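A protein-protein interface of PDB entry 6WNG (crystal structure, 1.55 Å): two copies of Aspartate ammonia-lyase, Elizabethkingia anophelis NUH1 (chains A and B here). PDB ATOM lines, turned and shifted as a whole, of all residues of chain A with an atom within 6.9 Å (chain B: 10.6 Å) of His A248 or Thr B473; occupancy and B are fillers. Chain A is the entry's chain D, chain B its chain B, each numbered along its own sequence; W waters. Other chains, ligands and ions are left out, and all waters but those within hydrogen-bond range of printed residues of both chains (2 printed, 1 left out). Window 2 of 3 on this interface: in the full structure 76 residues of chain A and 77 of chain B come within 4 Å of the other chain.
Of the 13 printed residues of chain B, 5 touch a printed residue of chain A.
Printed residues of chain B that touch a printed residue of chain A: Ala B420, Pro B423, Pro B471, His B472 and Thr B473.
Hydrophobic or aromatic side chains of chain B that line the printed part of chain A: Pro B423 and Pro B471.
Of the 15 printed residues of chain A, 5 touch a printed residue of chain B.
Hydrophobic or aromatic side chains of chain A within 4 Å of the printed part of chain B: His A248 and Pro A249.
No position is printed for both chains.
Among the printed residues, pairs that only touch across the chains: Gly A244 with Pro B471 (3.3 Å), Asn A246 with Ala B420 (3.5 Å), Asn A246 with Pro B423 (3.6 Å), Ala A247 with Pro B471 (3.1 Å), His A248 with Pro B471 (3.9 Å), His A248 with His B472 (3.8 Å), His A248 with Thr B473 (3.7 Å), Pro A249 with Pro B471 (3.8 Å), Pro A249 with His B472 (3.6 Å) and Pro A249 with Thr B473 (3.7 Å).
The side-chain amino group of Lys B474 sits at hydrogen-bond distance from the backbone carbonyl oxygen of Pro B423 (2.9 Å).
O of Asn B467 sits close to NE2 of His B472.
The backbone NH of Asp A250 sits at hydrogen-bond distance from a ring nitrogen (ND1) of His A248, at 2.9 Å.
Water W2 lies within hydrogen-bond range of OD1 of Asn A246 (2.7 Å) and O of Ala B420 (2.7 Å).
Water W1 lies within hydrogen-bond range of O of Asn B470 (2.9 Å), N of Asn A246 (3.0 Å) and N of His B472 (3.5 Å).
Of chain B, only Pro B471 (3.9 Å), His B472 (3.8 Å) and Thr B473 (3.7 Å) come within 4 Å of His A248.
Thr B473 touches just these residues of chain A: His A248 (3.7 Å) and Pro A249 (3.7 Å).
Of chain B, only Pro B471 and His B472 come within 4 Å of Ala A247.
No residue of chain B comes within 4 Å of Asp A250.
Of the printed residues of chain B, Gly A244 touches Pro B471 (3.3 Å).
Of the printed residues of chain A, Pro B423 touches Asn A246 (3.6 Å).
The nearest residue of chain A that does not touch Thr B473 is Ala A247 (5.2 Å).
The backbone NH (N) of His B472 is in hydrogen-bond range of the backbone carbonyl oxygen (O) of Ala A247 (3.0 Å).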
ATOM      1  N   ASN A  69      -0.014  25.008   3.117  1.00  0.00           N
ATOM      2  CA  ASN A  69       1.301  25.489   3.535  1.00  0.00           C
ATOM      3  C   ASN A  69       1.415  25.512   5.051  1.00  0.00           C
ATOM      4  O   ASN A  69       2.454  25.147   5.615  1.00  0.00           O
ATOM      5  CB  ASN A  69       1.563  26.882   2.963  1.00  0.00           C
ATOM      6  CG  ASN A  69       1.918  26.855   1.486  1.00  0.00           C
ATOM      7  OD1 ASN A  69       2.651  25.980   1.031  1.00  0.00           O
ATOM      8  ND2 ASN A  69       1.405  27.820   0.733  1.00  0.00           N
ATOM      9  N   LEU A  72       1.880  21.963   6.348  1.00  0.00           N
ATOM     10  CA  LEU A  72       3.202  21.431   6.050  1.00  0.00           C
ATOM     11  C   LEU A  72       4.310  22.153   6.804  1.00  0.00           C
ATOM     12  O   LEU A  72       5.491  21.873   6.564  1.00  0.00           O
ATOM     13  CB  LEU A  72       3.471  21.495   4.544  1.00  0.00           C
ATOM     14  CG  LEU A  72       2.575  20.594   3.695  1.00  0.00           C
ATOM     15  CD1 LEU A  72       2.736  20.887   2.208  1.00  0.00           C
ATOM     16  CD2 LEU A  72       2.868  19.132   4.006  1.00  0.00           C
ATOM     17  N   LEU A  74       5.111  25.348   6.625  1.00  0.00           N
ATOM     18  CA  LEU A  74       5.756  26.358   5.799  1.00  0.00           C
ATOM     19  C   LEU A  74       5.196  27.759   6.004  1.00  0.00           C
ATOM     20  O   LEU A  74       5.806  28.721   5.525  1.00  0.00           O
ATOM     21  CB  LEU A  74       5.631  25.994   4.310  1.00  0.00           C
ATOM     22  CG  LEU A  74       6.150  24.615   3.898  1.00  0.00           C
ATOM     23  CD1 LEU A  74       5.763  24.326   2.454  1.00  0.00           C
ATOM     24  CD2 LEU A  74       7.661  24.550   4.084  1.00  0.00           C
ATOM     25  N   SER A 147       4.348  28.571  -2.510  1.00  0.00           N
ATOM     26  CA  SER A 147       4.253  27.254  -3.146  1.00  0.00           C
ATOM     27  C   SER A 147       3.458  27.266  -4.441  1.00  0.00           C
ATOM     28  O   SER A 147       3.151  26.189  -4.965  1.00  0.00           O
ATOM     29  CB  SER A 147       3.652  26.190  -2.219  1.00  0.00           C
ATOM     30  OG  SER A 147       4.336  26.143  -0.971  1.00  0.00           O
ATOM     31  N   GLY A 237       0.232  22.528  -7.437  1.00  0.00           N
ATOM     32  CA  GLY A 237       1.505  21.874  -7.219  1.00  0.00           C
ATOM     33  C   GLY A 237       2.384  21.821  -8.450  1.00  0.00           C
ATOM     34  O   GLY A 237       3.552  21.432  -8.339  1.00  0.00           O
ATOM     35  N   GLY A 244       6.849  21.140 -10.257  1.00  0.00           N
ATOM     36  CA  GLY A 244       6.716  21.270  -8.816  1.00  0.00           C
ATOM     37  C   GLY A 244       7.880  21.935  -8.116  1.00  0.00           C
ATOM     38  O   GLY A 244       7.971  21.849  -6.885  1.00  0.00           O
ATOM     39  N   LEU A 245       8.775  22.589  -8.858  1.00  0.00           N
ATOM     40  CA  LEU A 245       9.879  23.311  -8.238  1.00  0.00           C
ATOM     41  C   LEU A 245       9.355  24.257  -7.167  1.00  0.00           C
ATOM     42  O   LEU A 245       8.423  25.036  -7.410  1.00  0.00           O
ATOM     43  CB  LEU A 245      10.655  24.090  -9.301  1.00  0.00           C
ATOM     44  CG  LEU A 245      11.958  24.733  -8.799  1.00  0.00           C
ATOM     45  CD1 LEU A 245      13.043  23.677  -8.554  1.00  0.00           C
ATOM     46  CD2 LEU A 245      12.464  25.777  -9.794  1.00  0.00           C
ATOM     47  N   ASN A 246       9.940  24.148  -5.974  1.00  0.00           N
ATOM     48  CA  ASN A 246       9.681  24.907  -4.754  1.00  0.00           C
ATOM     49  C   ASN A 246       8.508  24.353  -3.951  1.00  0.00           C
ATOM     50  O   ASN A 246       8.325  24.770  -2.801  1.00  0.00           O
ATOM     51  CB  ASN A 246       9.464  26.413  -5.005  1.00  0.00           C
ATOM     52  CG  ASN A 246      10.713  27.084  -5.534  1.00  0.00           C
ATOM     53  OD1 ASN A 246      11.791  26.478  -5.556  1.00  0.00           O
ATOM     54  ND2 ASN A 246      10.582  28.328  -5.974  1.00  0.00           N
ATOM     55  N   ALA A 247       7.739  23.406  -4.474  1.00  0.00           N
ATOM     56  CA  ALA A 247       6.677  22.805  -3.681  1.00  0.00           C
ATOM     57  C   ALA A 247       7.217  21.664  -2.823  1.00  0.00           C
ATOM     58  O   ALA A 247       8.192  21.000  -3.175  1.00  0.00           O
ATOM     59  CB  ALA A 247       5.559  22.297  -4.592  1.00  0.00           C
ATOM     60  N   HIS A 248       6.577  21.459  -1.673  1.00  0.00           N
ATOM     61  CA  HIS A 248       6.838  20.282  -0.850  1.00  0.00           C
ATOM     62  C   HIS A 248       6.290  19.044  -1.563  1.00  0.00           C
ATOM     63  O   HIS A 248       5.255  19.131  -2.226  1.00  0.00           O
ATOM     64  CB  HIS A 248       6.155  20.472   0.506  1.00  0.00           C
ATOM     65  CG  HIS A 248       6.460  19.409   1.514  1.00  0.00           C
ATOM     66  ND1 HIS A 248       5.876  18.161   1.476  1.00  0.00           N
ATOM     67  CD2 HIS A 248       7.243  19.425   2.619  1.00  0.00           C
ATOM     68  CE1 HIS A 248       6.310  17.444   2.499  1.00  0.00           C
ATOM     69  NE2 HIS A 248       7.139  18.189   3.207  1.00  0.00           N
ATOM     70  N   PRO A 249       6.950  17.886  -1.455  1.00  0.00           N
ATOM     71  CA  PRO A 249       6.454  16.699  -2.184  1.00  0.00           C
ATOM     72  C   PRO A 249       5.032  16.285  -1.826  1.00  0.00           C
ATOM     73  O   PRO A 249       4.380  15.630  -2.649  1.00  0.00           O
ATOM     74  CB  PRO A 249       7.460  15.600  -1.799  1.00  0.00           C
ATOM     75  CG  PRO A 249       8.713  16.352  -1.454  1.00  0.00           C
ATOM     76  CD  PRO A 249       8.240  17.621  -0.788  1.00  0.00           C
ATOM     77  N   ASP A 250       4.535  16.628  -0.639  1.00  0.00           N
ATOM     78  CA  ASP A 250       3.173  16.291  -0.238  1.00  0.00           C
ATOM     79  C   ASP A 250       2.162  17.380  -0.582  1.00  0.00           C
ATOM     80  O   ASP A 250       0.960  17.193  -0.353  1.00  0.00           O
ATOM     81  CB  ASP A 250       3.128  16.001   1.266  1.00  0.00           C
ATOM     82  CG  ASP A 250       3.894  14.751   1.638  1.00  0.00           C
ATOM     83  OD1 ASP A 250       4.052  13.871   0.769  1.00  0.00           O
ATOM     84  OD2 ASP A 250       4.320  14.653   2.807  1.00  0.00           O
ATOM     85  N   TYR A 251       2.612  18.498  -1.145  1.00  0.00           N
ATOM     86  CA  TYR A 251       1.732  19.652  -1.306  1.00  0.00           C
ATOM     87  C   TYR A 251       0.654  19.424  -2.368  1.00  0.00           C
ATOM     88  O   TYR A 251      -0.498  19.824  -2.171  1.00  0.00           O
ATOM     89  CB  TYR A 251       2.571  20.888  -1.629  1.00  0.00           C
ATOM     90  CG  TYR A 251       1.777  22.093  -2.087  1.00  0.00           C
ATOM     91  CD1 TYR A 251       1.488  22.276  -3.434  1.00  0.00           C
ATOM     92  CD2 TYR A 251       1.329  23.048  -1.181  1.00  0.00           C
ATOM     93  CE1 TYR A 251       0.763  23.369  -3.865  1.00  0.00           C
ATOM     94  CE2 TYR A 251       0.604  24.164  -1.611  1.00  0.00           C
ATOM     95  CZ  TYR A 251       0.326  24.310  -2.953  1.00  0.00           C
ATOM     96  OH  TYR A 251      -0.379  25.407  -3.411  1.00  0.00           O
ATOM     97  N   ALA A 252       1.002  18.824  -3.511  1.00  0.00           N
ATOM     98  CA  ALA A 252       0.039  18.746  -4.611  1.00  0.00           C
ATOM     99  C   ALA A 252      -1.209  17.977  -4.192  1.00  0.00           C
ATOM    100  O   ALA A 252      -2.342  18.420  -4.431  1.00  0.00           O
ATOM    101  CB  ALA A 252       0.687  18.102  -5.839  1.00  0.00           C
ATOM    102  N   VAL A 253      -1.018  16.832  -3.536  1.00  0.00           N
ATOM    103  CA  VAL A 253      -2.150  16.021  -3.100  1.00  0.00           C
ATOM    104  C   VAL A 253      -2.907  16.717  -1.977  1.00  0.00           C
ATOM    105  O   VAL A 253      -4.138  16.821  -2.011  1.00  0.00           O
ATOM    106  CB  VAL A 253      -1.670  14.623  -2.670  1.00  0.00           C
ATOM    107  CG1 VAL A 253      -2.767  13.895  -1.894  1.00  0.00           C
ATOM    108  CG2 VAL A 253      -1.237  13.816  -3.896  1.00  0.00           C
ATOM    109  N   ALA B 420      14.810  28.504  -7.753  1.00  0.00           N
ATOM    110  CA  ALA B 420      14.962  27.465  -6.736  1.00  0.00           C
ATOM    111  C   ALA B 420      15.408  28.011  -5.384  1.00  0.00           C
ATOM    112  O   ALA B 420      15.302  27.299  -4.380  1.00  0.00           O
ATOM    113  CB  ALA B 420      15.965  26.410  -7.209  1.00  0.00           C
ATOM    114  N   PRO B 423      12.532  29.622  -1.669  1.00  0.00           N
ATOM    115  CA  PRO B 423      12.162  29.141  -0.326  1.00  0.00           C
ATOM    116  C   PRO B 423      13.205  29.437   0.722  1.00  0.00           C
ATOM    117  O   PRO B 423      12.895  29.366   1.912  1.00  0.00           O
ATOM    118  CB  PRO B 423      11.984  27.628  -0.520  1.00  0.00           C
ATOM    119  CG  PRO B 423      11.704  27.469  -1.973  1.00  0.00           C
ATOM    120  CD  PRO B 423      12.549  28.518  -2.646  1.00  0.00           C
ATOM    121  N   TYR B 424      14.430  29.767   0.317  1.00  0.00           N
ATOM    122  CA  TYR B 424      15.520  29.994   1.252  1.00  0.00           C
ATOM    123  C   TYR B 424      15.833  31.466   1.473  1.00  0.00           C
ATOM    124  O   TYR B 424      16.182  31.853   2.594  1.00  0.00           O
ATOM    125  CB  TYR B 424      16.778  29.264   0.762  1.00  0.00           C
ATOM    126  CG  TYR B 424      16.617  27.757   0.798  1.00  0.00           C
ATOM    127  CD1 TYR B 424      16.837  27.049   1.971  1.00  0.00           C
ATOM    128  CD2 TYR B 424      16.211  27.049  -0.331  1.00  0.00           C
ATOM    129  CE1 TYR B 424      16.681  25.671   2.021  1.00  0.00           C
ATOM    130  CE2 TYR B 424      16.052  25.665  -0.293  1.00  0.00           C
ATOM    131  CZ  TYR B 424      16.292  24.987   0.892  1.00  0.00           C
ATOM    132  OH  TYR B 424      16.136  23.618   0.959  1.00  0.00           O
ATOM    133  N   LYS B 458      25.255  24.189   0.564  1.00  0.00           N
ATOM    134  CA  LYS B 458      23.818  24.192   0.316  1.00  0.00           C
ATOM    135  C   LYS B 458      23.503  24.657  -1.103  1.00  0.00           C
ATOM    136  O   LYS B 458      22.650  24.074  -1.777  1.00  0.00           O
ATOM    137  CB  LYS B 458      23.098  25.063   1.352  1.00  0.00           C
ATOM    138  CG  LYS B 458      21.592  25.128   1.125  1.00  0.00           C
ATOM    139  CD  LYS B 458      20.855  25.757   2.303  1.00  0.00           C
ATOM    140  CE  LYS B 458      20.238  24.693   3.181  1.00  0.00           C
ATOM    141  NZ  LYS B 458      19.838  25.264   4.494  1.00  0.00           N
ATOM    142  N   GLU B 461      23.861  22.079  -3.799  1.00  0.00           N
ATOM    143  CA  GLU B 461      22.744  21.142  -3.877  1.00  0.00           C
ATOM    144  C   GLU B 461      21.554  21.764  -4.605  1.00  0.00           C
ATOM    145  O   GLU B 461      20.974  21.151  -5.510  1.00  0.00           O
ATOM    146  CB  GLU B 461      22.340  20.704  -2.462  1.00  0.00           C
ATOM    147  CG  GLU B 461      21.485  19.436  -2.390  1.00  0.00           C
ATOM    148  CD  GLU B 461      20.001  19.662  -2.648  1.00  0.00           C
ATOM    149  OE1 GLU B 461      19.542  20.831  -2.751  1.00  0.00           O
ATOM    150  OE2 GLU B 461      19.282  18.643  -2.732  1.00  0.00           O
ATOM    151  N   ILE B 462      21.167  22.979  -4.213  1.00  0.00           N
ATOM    152  CA  ILE B 462      19.907  23.544  -4.698  1.00  0.00           C
ATOM    153  C   ILE B 462      19.987  23.842  -6.190  1.00  0.00           C
ATOM    154  O   ILE B 462      19.011  23.652  -6.927  1.00  0.00           O
ATOM    155  CB  ILE B 462      19.546  24.807  -3.900  1.00  0.00           C
ATOM    156  CG1 ILE B 462      19.364  24.497  -2.411  1.00  0.00           C
ATOM    157  CG2 ILE B 462      18.276  25.448  -4.474  1.00  0.00           C
ATOM    158  CD1 ILE B 462      19.452  25.743  -1.534  1.00  0.00           C
ATOM    159  N   ASN B 467      18.554  18.504  -9.366  1.00  0.00           N
ATOM    160  CA  ASN B 467      17.730  18.762  -8.191  1.00  0.00           C
ATOM    161  C   ASN B 467      16.679  19.826  -8.435  1.00  0.00           C
ATOM    162  O   ASN B 467      16.002  20.238  -7.491  1.00  0.00           O
ATOM    163  CB  ASN B 467      18.605  19.161  -7.005  1.00  0.00           C
ATOM    164  CG  ASN B 467      19.488  18.034  -6.554  1.00  0.00           C
ATOM    165  OD1 ASN B 467      19.135  16.859  -6.721  1.00  0.00           O
ATOM    166  ND2 ASN B 467      20.654  18.370  -6.008  1.00  0.00           N
ATOM    167  N   ASN B 470      11.800  18.430  -9.583  1.00  0.00           N
ATOM    168  CA  ASN B 470      10.788  17.786  -8.760  1.00  0.00           C
ATOM    169  C   ASN B 470      10.508  18.685  -7.574  1.00  0.00           C
ATOM    170  O   ASN B 470      11.338  19.532  -7.227  1.00  0.00           O
ATOM    171  CB  ASN B 470      11.260  16.423  -8.229  1.00  0.00           C
ATOM    172  CG  ASN B 470      11.671  15.474  -9.319  1.00  0.00           C
ATOM    173  OD1 ASN B 470      10.870  14.658  -9.790  1.00  0.00           O
ATOM    174  ND2 ASN B 470      12.925  15.564  -9.728  1.00  0.00           N
ATOM    175  N   PRO B 471       9.378  18.489  -6.891  1.00  0.00           N
ATOM    176  CA  PRO B 471       9.234  19.064  -5.550  1.00  0.00           C
ATOM    177  C   PRO B 471      10.269  18.462  -4.608  1.00  0.00           C
ATOM    178  O   PRO B 471      10.715  17.327  -4.788  1.00  0.00           O
ATOM    179  CB  PRO B 471       7.805  18.674  -5.143  1.00  0.00           C
ATOM    180  CG  PRO B 471       7.454  17.502  -6.001  1.00  0.00           C
ATOM    181  CD  PRO B 471       8.193  17.715  -7.300  1.00  0.00           C
ATOM    182  N   HIS B 472      10.639  19.235  -3.582  1.00  0.00           N
ATOM    183  CA  HIS B 472      11.638  18.811  -2.608  1.00  0.00           C
ATOM    184  C   HIS B 472      11.303  19.362  -1.230  1.00  0.00           C
ATOM    185  O   HIS B 472      10.643  20.401  -1.095  1.00  0.00           O
ATOM    186  CB  HIS B 472      13.055  19.266  -3.005  1.00  0.00           C
ATOM    187  CG  HIS B 472      13.617  18.525  -4.178  1.00  0.00           C
ATOM    188  ND1 HIS B 472      13.891  17.176  -4.136  1.00  0.00           N
ATOM    189  CD2 HIS B 472      13.958  18.943  -5.422  1.00  0.00           C
ATOM    190  CE1 HIS B 472      14.373  16.791  -5.305  1.00  0.00           C
ATOM    191  NE2 HIS B 472      14.420  17.841  -6.104  1.00  0.00           N
ATOM    192  N   THR B 473      11.792  18.661  -0.208  1.00  0.00           N
ATOM    193  CA  THR B 473      11.788  19.170   1.152  1.00  0.00           C
ATOM    194  C   THR B 473      12.964  20.115   1.363  1.00  0.00           C
ATOM    195  O   THR B 473      14.032  19.964   0.759  1.00  0.00           O
ATOM    196  CB  THR B 473      11.851  18.019   2.157  1.00  0.00           C
ATOM    197  OG1 THR B 473      12.948  17.159   1.832  1.00  0.00           O
ATOM    198  CG2 THR B 473      10.567  17.214   2.110  1.00  0.00           C
ATOM    199  N   LYS B 474      12.756  21.104   2.222  1.00  0.00           N
ATOM    200  CA  LYS B 474      13.826  22.020   2.579  1.00  0.00           C
ATOM    201  C   LYS B 474      14.754  21.372   3.593  1.00  0.00           C
ATOM    202  O   LYS B 474      14.358  20.486   4.359  1.00  0.00           O
ATOM    203  CB  LYS B 474      13.270  23.317   3.163  1.00  0.00           C
ATOM    204  CG  LYS B 474      12.500  24.161   2.146  1.00  0.00           C
ATOM    205  CD  LYS B 474      11.814  25.336   2.837  1.00  0.00           C
ATOM    206  CE  LYS B 474      12.813  26.394   3.282  1.00  0.00           C
ATOM    207  NZ  LYS B 474      12.167  27.538   4.006  1.00  0.00           N
ATOM    208  N   PHE B 475      15.992  21.832   3.599  1.00  0.00           N
ATOM    209  CA  PHE B 475      16.973  21.313   4.535  1.00  0.00           C
ATOM    210  C   PHE B 475      17.868  22.446   5.003  1.00  0.00           C
ATOM    211  O   PHE B 475      17.601  23.615   4.707  1.00  0.00           O
ATOM    212  CB  PHE B 475      17.791  20.181   3.889  1.00  0.00           C
ATOM    213  CG  PHE B 475      18.602  20.617   2.690  1.00  0.00           C
ATOM    214  CD1 PHE B 475      17.991  20.881   1.472  1.00  0.00           C
ATOM    215  CD2 PHE B 475      19.981  20.747   2.786  1.00  0.00           C
ATOM    216  CE1 PHE B 475      18.738  21.283   0.370  1.00  0.00           C
ATOM    217  CE2 PHE B 475      20.733  21.152   1.687  1.00  0.00           C
ATOM    218  CZ  PHE B 475      20.113  21.417   0.483  1.00  0.00           C
ATOM    219  OXT PHE B 475      18.853  22.229   5.710  1.00  0.00           O
HETATM  220  O   HOH W   1      11.763  21.843  -5.583  1.00  0.00           O
HETATM  221  O   HOH W   2      13.617  25.211  -4.060  1.00  0.00           O
